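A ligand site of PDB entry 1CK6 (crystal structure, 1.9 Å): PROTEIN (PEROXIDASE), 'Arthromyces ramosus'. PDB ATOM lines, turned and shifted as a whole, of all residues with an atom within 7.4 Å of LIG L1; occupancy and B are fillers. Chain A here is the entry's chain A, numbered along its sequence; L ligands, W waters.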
ATOM      1  N   ARG A  52      17.144   9.825   3.840  1.00  0.00           N
ATOM      2  CA  ARG A  52      16.504  11.134   3.661  1.00  0.00           C
ATOM      3  C   ARG A  52      15.168  10.891   2.941  1.00  0.00           C
ATOM      4  O   ARG A  52      14.135  11.460   3.325  1.00  0.00           O
ATOM      5  CB  ARG A  52      17.487  11.996   2.875  1.00  0.00           C
ATOM      6  CG  ARG A  52      17.068  13.413   2.759  1.00  0.00           C
ATOM      7  CD  ARG A  52      18.167  14.273   2.147  1.00  0.00           C
ATOM      8  NE  ARG A  52      17.475  15.443   1.608  1.00  0.00           N
ATOM      9  CZ  ARG A  52      17.750  15.949   0.400  1.00  0.00           C
ATOM     10  NH1 ARG A  52      18.704  15.448  -0.408  1.00  0.00           N
ATOM     11  NH2 ARG A  52      16.961  16.918  -0.068  1.00  0.00           N
ATOM     12  N   PHE A  55      12.181   9.492   5.327  1.00  0.00           N
ATOM     13  CA  PHE A  55      11.702  10.593   6.138  1.00  0.00           C
ATOM     14  C   PHE A  55      10.835  11.455   5.239  1.00  0.00           C
ATOM     15  O   PHE A  55       9.677  11.674   5.602  1.00  0.00           O
ATOM     16  CB  PHE A  55      12.883  11.447   6.701  1.00  0.00           C
ATOM     17  CG  PHE A  55      12.465  12.700   7.478  1.00  0.00           C
ATOM     18  CD1 PHE A  55      11.397  12.684   8.391  1.00  0.00           C
ATOM     19  CD2 PHE A  55      13.147  13.899   7.269  1.00  0.00           C
ATOM     20  CE1 PHE A  55      11.017  13.839   9.074  1.00  0.00           C
ATOM     21  CE2 PHE A  55      12.772  15.054   7.944  1.00  0.00           C
ATOM     22  CZ  PHE A  55      11.707  15.024   8.846  1.00  0.00           C
ATOM     23  N   HIS A  56      11.270  11.889   4.053  1.00  0.00           N
ATOM     24  CA  HIS A  56      10.450  12.779   3.238  1.00  0.00           C
ATOM     25  C   HIS A  56       9.164  12.162   2.728  1.00  0.00           C
ATOM     26  O   HIS A  56       8.149  12.844   2.473  1.00  0.00           O
ATOM     27  CB  HIS A  56      11.303  13.319   2.062  1.00  0.00           C
ATOM     28  CG  HIS A  56      12.370  14.310   2.536  1.00  0.00           C
ATOM     29  ND1 HIS A  56      13.123  15.123   1.703  1.00  0.00           N
ATOM     30  CD2 HIS A  56      12.723  14.553   3.882  1.00  0.00           C
ATOM     31  CE1 HIS A  56      13.909  15.855   2.535  1.00  0.00           C
ATOM     32  NE2 HIS A  56      13.689  15.558   3.779  1.00  0.00           N
ATOM     33  N   ILE A  59       6.810  11.600   6.367  1.00  0.00           N
ATOM     34  CA  ILE A  59       6.358  12.828   7.019  1.00  0.00           C
ATOM     35  C   ILE A  59       5.285  13.605   6.230  1.00  0.00           C
ATOM     36  O   ILE A  59       4.711  14.544   6.799  1.00  0.00           O
ATOM     37  CB  ILE A  59       7.657  13.711   7.356  1.00  0.00           C
ATOM     38  CG1 ILE A  59       7.385  14.537   8.593  1.00  0.00           C
ATOM     39  CG2 ILE A  59       8.019  14.711   6.238  1.00  0.00           C
ATOM     40  CD1 ILE A  59       7.172  13.699   9.857  1.00  0.00           C
ATOM     41  N   PHE A  90       9.401  20.130  -4.629  1.00  0.00           N
ATOM     42  CA  PHE A  90       9.409  20.791  -3.328  1.00  0.00           C
ATOM     43  C   PHE A  90      10.872  21.117  -3.014  1.00  0.00           C
ATOM     44  O   PHE A  90      11.757  20.307  -3.316  1.00  0.00           O
ATOM     45  CB  PHE A  90       8.908  19.904  -2.204  1.00  0.00           C
ATOM     46  CG  PHE A  90       7.490  19.359  -2.253  1.00  0.00           C
ATOM     47  CD1 PHE A  90       6.542  19.884  -3.128  1.00  0.00           C
ATOM     48  CD2 PHE A  90       7.159  18.302  -1.396  1.00  0.00           C
ATOM     49  CE1 PHE A  90       5.251  19.325  -3.144  1.00  0.00           C
ATOM     50  CE2 PHE A  90       5.873  17.761  -1.434  1.00  0.00           C
ATOM     51  CZ  PHE A  90       4.914  18.267  -2.317  1.00  0.00           C
ATOM     52  N   PRO A  91      11.200  22.253  -2.387  1.00  0.00           N
ATOM     53  CA  PRO A  91      12.591  22.604  -2.078  1.00  0.00           C
ATOM     54  C   PRO A  91      13.272  21.659  -1.116  1.00  0.00           C
ATOM     55  O   PRO A  91      14.476  21.525  -1.197  1.00  0.00           O
ATOM     56  CB  PRO A  91      12.497  24.052  -1.601  1.00  0.00           C
ATOM     57  CG  PRO A  91      11.074  24.213  -1.110  1.00  0.00           C
ATOM     58  CD  PRO A  91      10.272  23.358  -2.075  1.00  0.00           C
ATOM     59  N   ALA A  92      12.551  20.961  -0.224  1.00  0.00           N
ATOM     60  CA  ALA A  92      13.157  19.998   0.682  1.00  0.00           C
ATOM     61  C   ALA A  92      13.645  18.767  -0.056  1.00  0.00           C
ATOM     62  O   ALA A  92      14.443  18.017   0.501  1.00  0.00           O
ATOM     63  CB  ALA A  92      12.146  19.505   1.700  1.00  0.00           C
ATOM     64  N   ASN A  93      13.229  18.540  -1.312  1.00  0.00           N
ATOM     65  CA  ASN A  93      13.513  17.322  -2.054  1.00  0.00           C
ATOM     66  C   ASN A  93      14.537  17.396  -3.138  1.00  0.00           C
ATOM     67  O   ASN A  93      14.532  16.573  -4.057  1.00  0.00           O
ATOM     68  CB  ASN A  93      12.226  16.793  -2.668  1.00  0.00           C
ATOM     69  CG  ASN A  93      11.365  16.034  -1.680  1.00  0.00           C
ATOM     70  OD1 ASN A  93      11.885  15.331  -0.808  1.00  0.00           O
ATOM     71  ND2 ASN A  93      10.052  16.126  -1.742  1.00  0.00           N
ATOM     72  N   GLY A  94      15.441  18.371  -3.087  1.00  0.00           N
ATOM     73  CA  GLY A  94      16.485  18.406  -4.081  1.00  0.00           C
ATOM     74  C   GLY A  94      17.509  17.294  -3.819  1.00  0.00           C
ATOM     75  O   GLY A  94      17.651  16.735  -2.722  1.00  0.00           O
ATOM     76  N   LEU A  96      17.430  14.237  -4.958  1.00  0.00           N
ATOM     77  CA  LEU A  96      16.878  12.932  -4.786  1.00  0.00           C
ATOM     78  C   LEU A  96      16.495  12.222  -6.054  1.00  0.00           C
ATOM     79  O   LEU A  96      16.420  10.989  -6.039  1.00  0.00           O
ATOM     80  CB  LEU A  96      15.689  13.057  -3.843  1.00  0.00           C
ATOM     81  CG  LEU A  96      16.042  13.479  -2.414  1.00  0.00           C
ATOM     82  CD1 LEU A  96      14.769  13.542  -1.608  1.00  0.00           C
ATOM     83  CD2 LEU A  96      17.058  12.527  -1.788  1.00  0.00           C
ATOM     84  N   ILE A 153       7.541  19.077   5.159  1.00  0.00           N
ATOM     85  CA  ILE A 153       8.857  18.595   5.509  1.00  0.00           C
ATOM     86  C   ILE A 153       9.634  19.680   6.250  1.00  0.00           C
ATOM     87  O   ILE A 153       9.773  20.773   5.699  1.00  0.00           O
ATOM     88  CB  ILE A 153       9.648  18.175   4.226  1.00  0.00           C
ATOM     89  CG1 ILE A 153       8.833  17.127   3.443  1.00  0.00           C
ATOM     90  CG2 ILE A 153      11.048  17.624   4.604  1.00  0.00           C
ATOM     91  CD1 ILE A 153       9.428  16.849   2.059  1.00  0.00           C
ATOM     92  N   PRO A 154      10.137  19.423   7.460  1.00  0.00           N
ATOM     93  CA  PRO A 154      10.990  20.355   8.224  1.00  0.00           C
ATOM     94  C   PRO A 154      12.246  20.768   7.455  1.00  0.00           C
ATOM     95  O   PRO A 154      12.895  19.964   6.751  1.00  0.00           O
ATOM     96  CB  PRO A 154      11.346  19.614   9.513  1.00  0.00           C
ATOM     97  CG  PRO A 154      10.222  18.647   9.659  1.00  0.00           C
ATOM     98  CD  PRO A 154       9.883  18.208   8.228  1.00  0.00           C
ATOM     99  N   GLY A 155      12.595  22.039   7.631  1.00  0.00           N
ATOM    100  CA  GLY A 155      13.742  22.602   6.964  1.00  0.00           C
ATOM    101  C   GLY A 155      14.814  23.022   7.956  1.00  0.00           C
ATOM    102  O   GLY A 155      14.512  23.368   9.108  1.00  0.00           O
ATOM    103  N   PRO A 156      16.083  23.088   7.519  1.00  0.00           N
ATOM    104  CA  PRO A 156      17.232  23.453   8.359  1.00  0.00           C
ATOM    105  C   PRO A 156      17.216  24.884   8.883  1.00  0.00           C
ATOM    106  O   PRO A 156      17.885  25.180   9.864  1.00  0.00           O
ATOM    107  CB  PRO A 156      18.415  23.134   7.492  1.00  0.00           C
ATOM    108  CG  PRO A 156      17.925  23.432   6.090  1.00  0.00           C
ATOM    109  CD  PRO A 156      16.504  22.881   6.128  1.00  0.00           C
ATOM    110  N   GLY A 157      16.462  25.788   8.255  1.00  0.00           N
ATOM    111  CA  GLY A 157      16.352  27.142   8.710  1.00  0.00           C
ATOM    112  C   GLY A 157      15.132  27.309   9.616  1.00  0.00           C
ATOM    113  O   GLY A 157      14.834  28.423  10.049  1.00  0.00           O
ATOM    114  N   ASN A 158      14.379  26.265   9.930  1.00  0.00           N
ATOM    115  CA  ASN A 158      13.196  26.435  10.763  1.00  0.00           C
ATOM    116  C   ASN A 158      13.535  26.575  12.227  1.00  0.00           C
ATOM    117  O   ASN A 158      14.572  26.094  12.667  1.00  0.00           O
ATOM    118  CB  ASN A 158      12.257  25.255  10.666  1.00  0.00           C
ATOM    119  CG  ASN A 158      11.545  25.031   9.363  1.00  0.00           C
ATOM    120  OD1 ASN A 158      10.956  23.968   9.162  1.00  0.00           O
ATOM    121  ND2 ASN A 158      11.533  25.889   8.368  1.00  0.00           N
ATOM    122  N   HIS A 184      21.321  11.383  11.320  1.00  0.00           N
ATOM    123  CA  HIS A 184      22.341  12.297  10.861  1.00  0.00           C
ATOM    124  C   HIS A 184      23.753  11.820  11.270  1.00  0.00           C
ATOM    125  O   HIS A 184      24.766  12.464  10.962  1.00  0.00           O
ATOM    126  CB  HIS A 184      22.061  13.691  11.412  1.00  0.00           C
ATOM    127  CG  HIS A 184      21.026  14.506  10.651  1.00  0.00           C
ATOM    128  ND1 HIS A 184      20.785  15.844  10.871  1.00  0.00           N
ATOM    129  CD2 HIS A 184      20.227  14.029   9.614  1.00  0.00           C
ATOM    130  CE1 HIS A 184      19.839  16.181   9.977  1.00  0.00           C
ATOM    131  NE2 HIS A 184      19.513  15.171   9.247  1.00  0.00           N
ATOM    132  N   GLY A 191      23.641  19.918  -1.041  1.00  0.00           N
ATOM    133  CA  GLY A 191      22.988  21.104  -1.551  1.00  0.00           C
ATOM    134  C   GLY A 191      22.922  22.322  -0.659  1.00  0.00           C
ATOM    135  O   GLY A 191      22.362  23.330  -1.106  1.00  0.00           O
ATOM    136  N   LEU A 192      23.389  22.312   0.580  1.00  0.00           N
ATOM    137  CA  LEU A 192      23.337  23.488   1.434  1.00  0.00           C
ATOM    138  C   LEU A 192      24.561  24.366   1.140  1.00  0.00           C
ATOM    139  O   LEU A 192      24.507  25.604   1.103  1.00  0.00           O
ATOM    140  CB  LEU A 192      23.272  22.953   2.850  1.00  0.00           C
ATOM    141  CG  LEU A 192      21.957  22.839   3.630  1.00  0.00           C
ATOM    142  CD1 LEU A 192      20.739  22.706   2.720  1.00  0.00           C
ATOM    143  CD2 LEU A 192      22.155  21.717   4.622  1.00  0.00           C
ATOM    144  N   PHE A 230      23.323  27.809   2.855  1.00  0.00           N
ATOM    145  CA  PHE A 230      22.010  27.940   3.417  1.00  0.00           C
ATOM    146  C   PHE A 230      21.926  27.172   4.751  1.00  0.00           C
ATOM    147  O   PHE A 230      22.293  25.982   4.858  1.00  0.00           O
ATOM    148  CB  PHE A 230      20.985  27.413   2.387  1.00  0.00           C
ATOM    149  CG  PHE A 230      19.580  27.602   2.903  1.00  0.00           C
ATOM    150  CD1 PHE A 230      19.079  28.897   3.092  1.00  0.00           C
ATOM    151  CD2 PHE A 230      18.815  26.490   3.298  1.00  0.00           C
ATOM    152  CE1 PHE A 230      17.829  29.067   3.688  1.00  0.00           C
ATOM    153  CE2 PHE A 230      17.564  26.682   3.892  1.00  0.00           C
ATOM    154  CZ  PHE A 230      17.071  27.959   4.088  1.00  0.00           C
ATOM    155  N   MET A 243      24.452  22.191  10.459  1.00  0.00           N
ATOM    156  CA  MET A 243      23.265  22.936  10.011  1.00  0.00           C
ATOM    157  C   MET A 243      22.546  23.503  11.231  1.00  0.00           C
ATOM    158  O   MET A 243      22.585  22.938  12.339  1.00  0.00           O
ATOM    159  CB  MET A 243      22.275  22.047   9.180  1.00  0.00           C
ATOM    160  CG  MET A 243      21.531  20.912   9.841  1.00  0.00           C
ATOM    161  SD  MET A 243      20.484  19.989   8.693  1.00  0.00           S
ATOM    162  CE  MET A 243      21.718  19.071   7.918  1.00  0.00           C
HETATM  163  C1  LIG L   1      15.528  20.006   3.536  1.00  0.00           C
HETATM  164  C2  LIG L   1      14.499  20.915   3.902  1.00  0.00           C
HETATM  165  C3  LIG L   1      14.446  22.202   3.389  1.00  0.00           C
HETATM  166  C4  LIG L   1      15.438  22.646   2.483  1.00  0.00           C
HETATM  167  C5  LIG L   1      16.467  21.786   2.091  1.00  0.00           C
HETATM  168  C6  LIG L   1      16.525  20.468   2.608  1.00  0.00           C
HETATM  169  O1  LIG L   1      17.519  19.636   2.176  1.00  0.00           O
HETATM  170  C7  LIG L   1      15.489  18.637   4.157  1.00  0.00           C
HETATM  171  O2  LIG L   1      16.200  17.685   3.703  1.00  0.00           O
HETATM  172  N1  LIG L   1      14.715  18.370   5.197  1.00  0.00           N
HETATM  173  O3  LIG L   1      14.719  17.079   5.723  1.00  0.00           O
HETATM  174  C1  LG2 L   2      20.585  15.268   5.297  1.00  0.00           C
HETATM  175  C2  LG2 L   2      17.471  18.400   7.251  1.00  0.00           C
HETATM  176  C3  LG2 L   2      15.607  14.891   9.938  1.00  0.00           C
HETATM  177  C4  LG2 L   2      18.184  11.688   7.446  1.00  0.00           C
HETATM  178  C5  LG2 L   2      19.900  16.442   5.601  1.00  0.00           C
HETATM  179  C6  LG2 L   2      20.087  17.705   4.919  1.00  0.00           C
HETATM  180  C7  LG2 L   2      19.195  18.576   5.464  1.00  0.00           C
HETATM  181  C8  LG2 L   2      18.454  17.846   6.453  1.00  0.00           C
HETATM  182  C9  LG2 L   2      19.018  20.053   5.153  1.00  0.00           C
HETATM  183  C10 LG2 L   2      21.104  17.966   3.824  1.00  0.00           C
HETATM  184  C11 LG2 L   2      20.677  17.465   2.455  1.00  0.00           C
HETATM  185  C12 LG2 L   2      21.645  17.897   1.381  1.00  0.00           C
HETATM  186  O1  LG2 L   2      22.297  17.062   0.780  1.00  0.00           O
HETATM  187  O2  LG2 L   2      21.786  19.095   1.154  1.00  0.00           O
HETATM  188  C13 LG2 L   2      16.783  17.744   8.254  1.00  0.00           C
HETATM  189  C14 LG2 L   2      15.821  18.369   9.128  1.00  0.00           C
HETATM  190  C15 LG2 L   2      15.298  17.393   9.900  1.00  0.00           C
HETATM  191  C16 LG2 L   2      15.988  16.162   9.527  1.00  0.00           C
HETATM  192  C17 LG2 L   2      15.459  19.837   9.216  1.00  0.00           C
HETATM  193  C18 LG2 L   2      14.210  17.563  10.779  1.00  0.00           C
HETATM  194  C19 LG2 L   2      14.271  17.633  12.224  1.00  0.00           C
HETATM  195  C20 LG2 L   2      16.081  13.688   9.426  1.00  0.00           C
HETATM  196  C21 LG2 L   2      15.500  12.392   9.726  1.00  0.00           C
HETATM  197  C22 LG2 L   2      16.173  11.487   8.968  1.00  0.00           C
HETATM  198  C23 LG2 L   2      17.183  12.240   8.230  1.00  0.00           C
HETATM  199  C24 LG2 L   2      14.349  12.158  10.707  1.00  0.00           C
HETATM  200  C25 LG2 L   2      15.939  10.102   8.781  1.00  0.00           C
HETATM  201  C26 LG2 L   2      15.403   9.156   9.717  1.00  0.00           C
HETATM  202  C27 LG2 L   2      19.168  12.383   6.739  1.00  0.00           C
HETATM  203  C28 LG2 L   2      20.306  11.786   6.083  1.00  0.00           C
HETATM  204  C29 LG2 L   2      20.950  12.782   5.477  1.00  0.00           C
HETATM  205  C30 LG2 L   2      20.265  14.006   5.792  1.00  0.00           C
HETATM  206  C31 LG2 L   2      20.744  10.324   6.177  1.00  0.00           C
HETATM  207  C32 LG2 L   2      22.192  12.659   4.636  1.00  0.00           C
HETATM  208  C33 LG2 L   2      21.947  12.613   3.128  1.00  0.00           C
HETATM  209  C34 LG2 L   2      23.238  12.523   2.323  1.00  0.00           C
HETATM  210  O3  LG2 L   2      23.196  12.599   1.102  1.00  0.00           O
HETATM  211  O4  LG2 L   2      24.309  12.373   2.906  1.00  0.00           O
HETATM  212  N1  LG2 L   2      18.875  16.531   6.530  1.00  0.00           N
HETATM  213  N2  LG2 L   2      16.919  16.394   8.518  1.00  0.00           N
HETATM  214  N3  LG2 L   2      17.092  13.589   8.487  1.00  0.00           N
HETATM  215  N4  LG2 L   2      19.202  13.758   6.627  1.00  0.00           N
HETATM  216 FE1  LG2 L   2      18.130  15.072   7.637  1.00  0.00          FE
HETATM  217  O   HOH W   1      16.601  19.899  -0.959  1.00  0.00           O
HETATM  218  O   HOH W   2      19.279  20.155  -0.044  1.00  0.00           O
HETATM  219  O   HOH W   3      16.429  14.998   5.387  1.00  0.00           O
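An oxygen (O2) of LIG L1 lies within hydrogen-bond range of the guanidinium group (NE) of Arg 52, at 3.3 Å. O of Pro 154 is in hydrogen-bond range of N1 of LIG L1, 2.9 Å away. A ring nitrogen (NE2) of His 184 binds an iron atom (FE1) of LG2 L2, 2.1 Å away. N of Gly 191 sits at hydrogen-bond distance from O2 of LG2 L2 (3.0 Å). O3 of LIG L1 sits at hydrogen-bond distance from NE2 of His 56 (2.7 Å).
Water W3 lies within hydrogen-bond range of O3 of LIG L1 and NE2 of His 56. Water W2 lies within hydrogen-bond range of O1 of LIG L1 (2.9 Å) and O2 of LG2 L2 (3.0 Å). Water W1 lies within hydrogen-bond range of O of Pro 91 (2.7 Å), N of Gly 94 (2.9 Å), NH2 of Arg 52 (3.1 Å), O of Ala 92 (3.2 Å) and O1 of LIG L1 (3.3 Å).
Phe 55 touches LIG L1 (CE2 to O3, 3.6 Å). Pro 91 touches LIG L1 (O to C5, 3.9 Å). Ala 92 touches LIG L1. CG2 of Ile 153 touches N1 of LIG L1, at 3.8 Å. Gly 155 touches LIG L1 (CA to C2, 3.6 Å). Pro 156 touches LIG L1. Hydrophobic or aromatic side chains within 4 Å of LIG L1: Phe 55, His 56, Ala 92, Ile 153 and Pro 156. Of the 21 residues printed, 9 come within 4 Å of LIG L1. The nearest printed residue that does not touch LIG L1 is Leu 192 (4.4 Å).
O of Ala 92 sits close to ND1 of His 56. The backbone NH (N) of Gly 155 lies within hydrogen-bond range of the side-chain amide oxygen (OD1) of Asn 158 (3.0 Å). The guanidinium group (NH2) of Arg 52 sits at hydrogen-bond distance from the backbone carbonyl oxygen (O) of Gly 94 (2.7 Å). The side-chain amide oxygen of Asn 93 lies within hydrogen-bond range of a ring nitrogen (ND1) of His 56, at 2.8 Å. O of Ala 92 sits at hydrogen-bond distance from NH2 of Arg 52 (2.8 Å).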
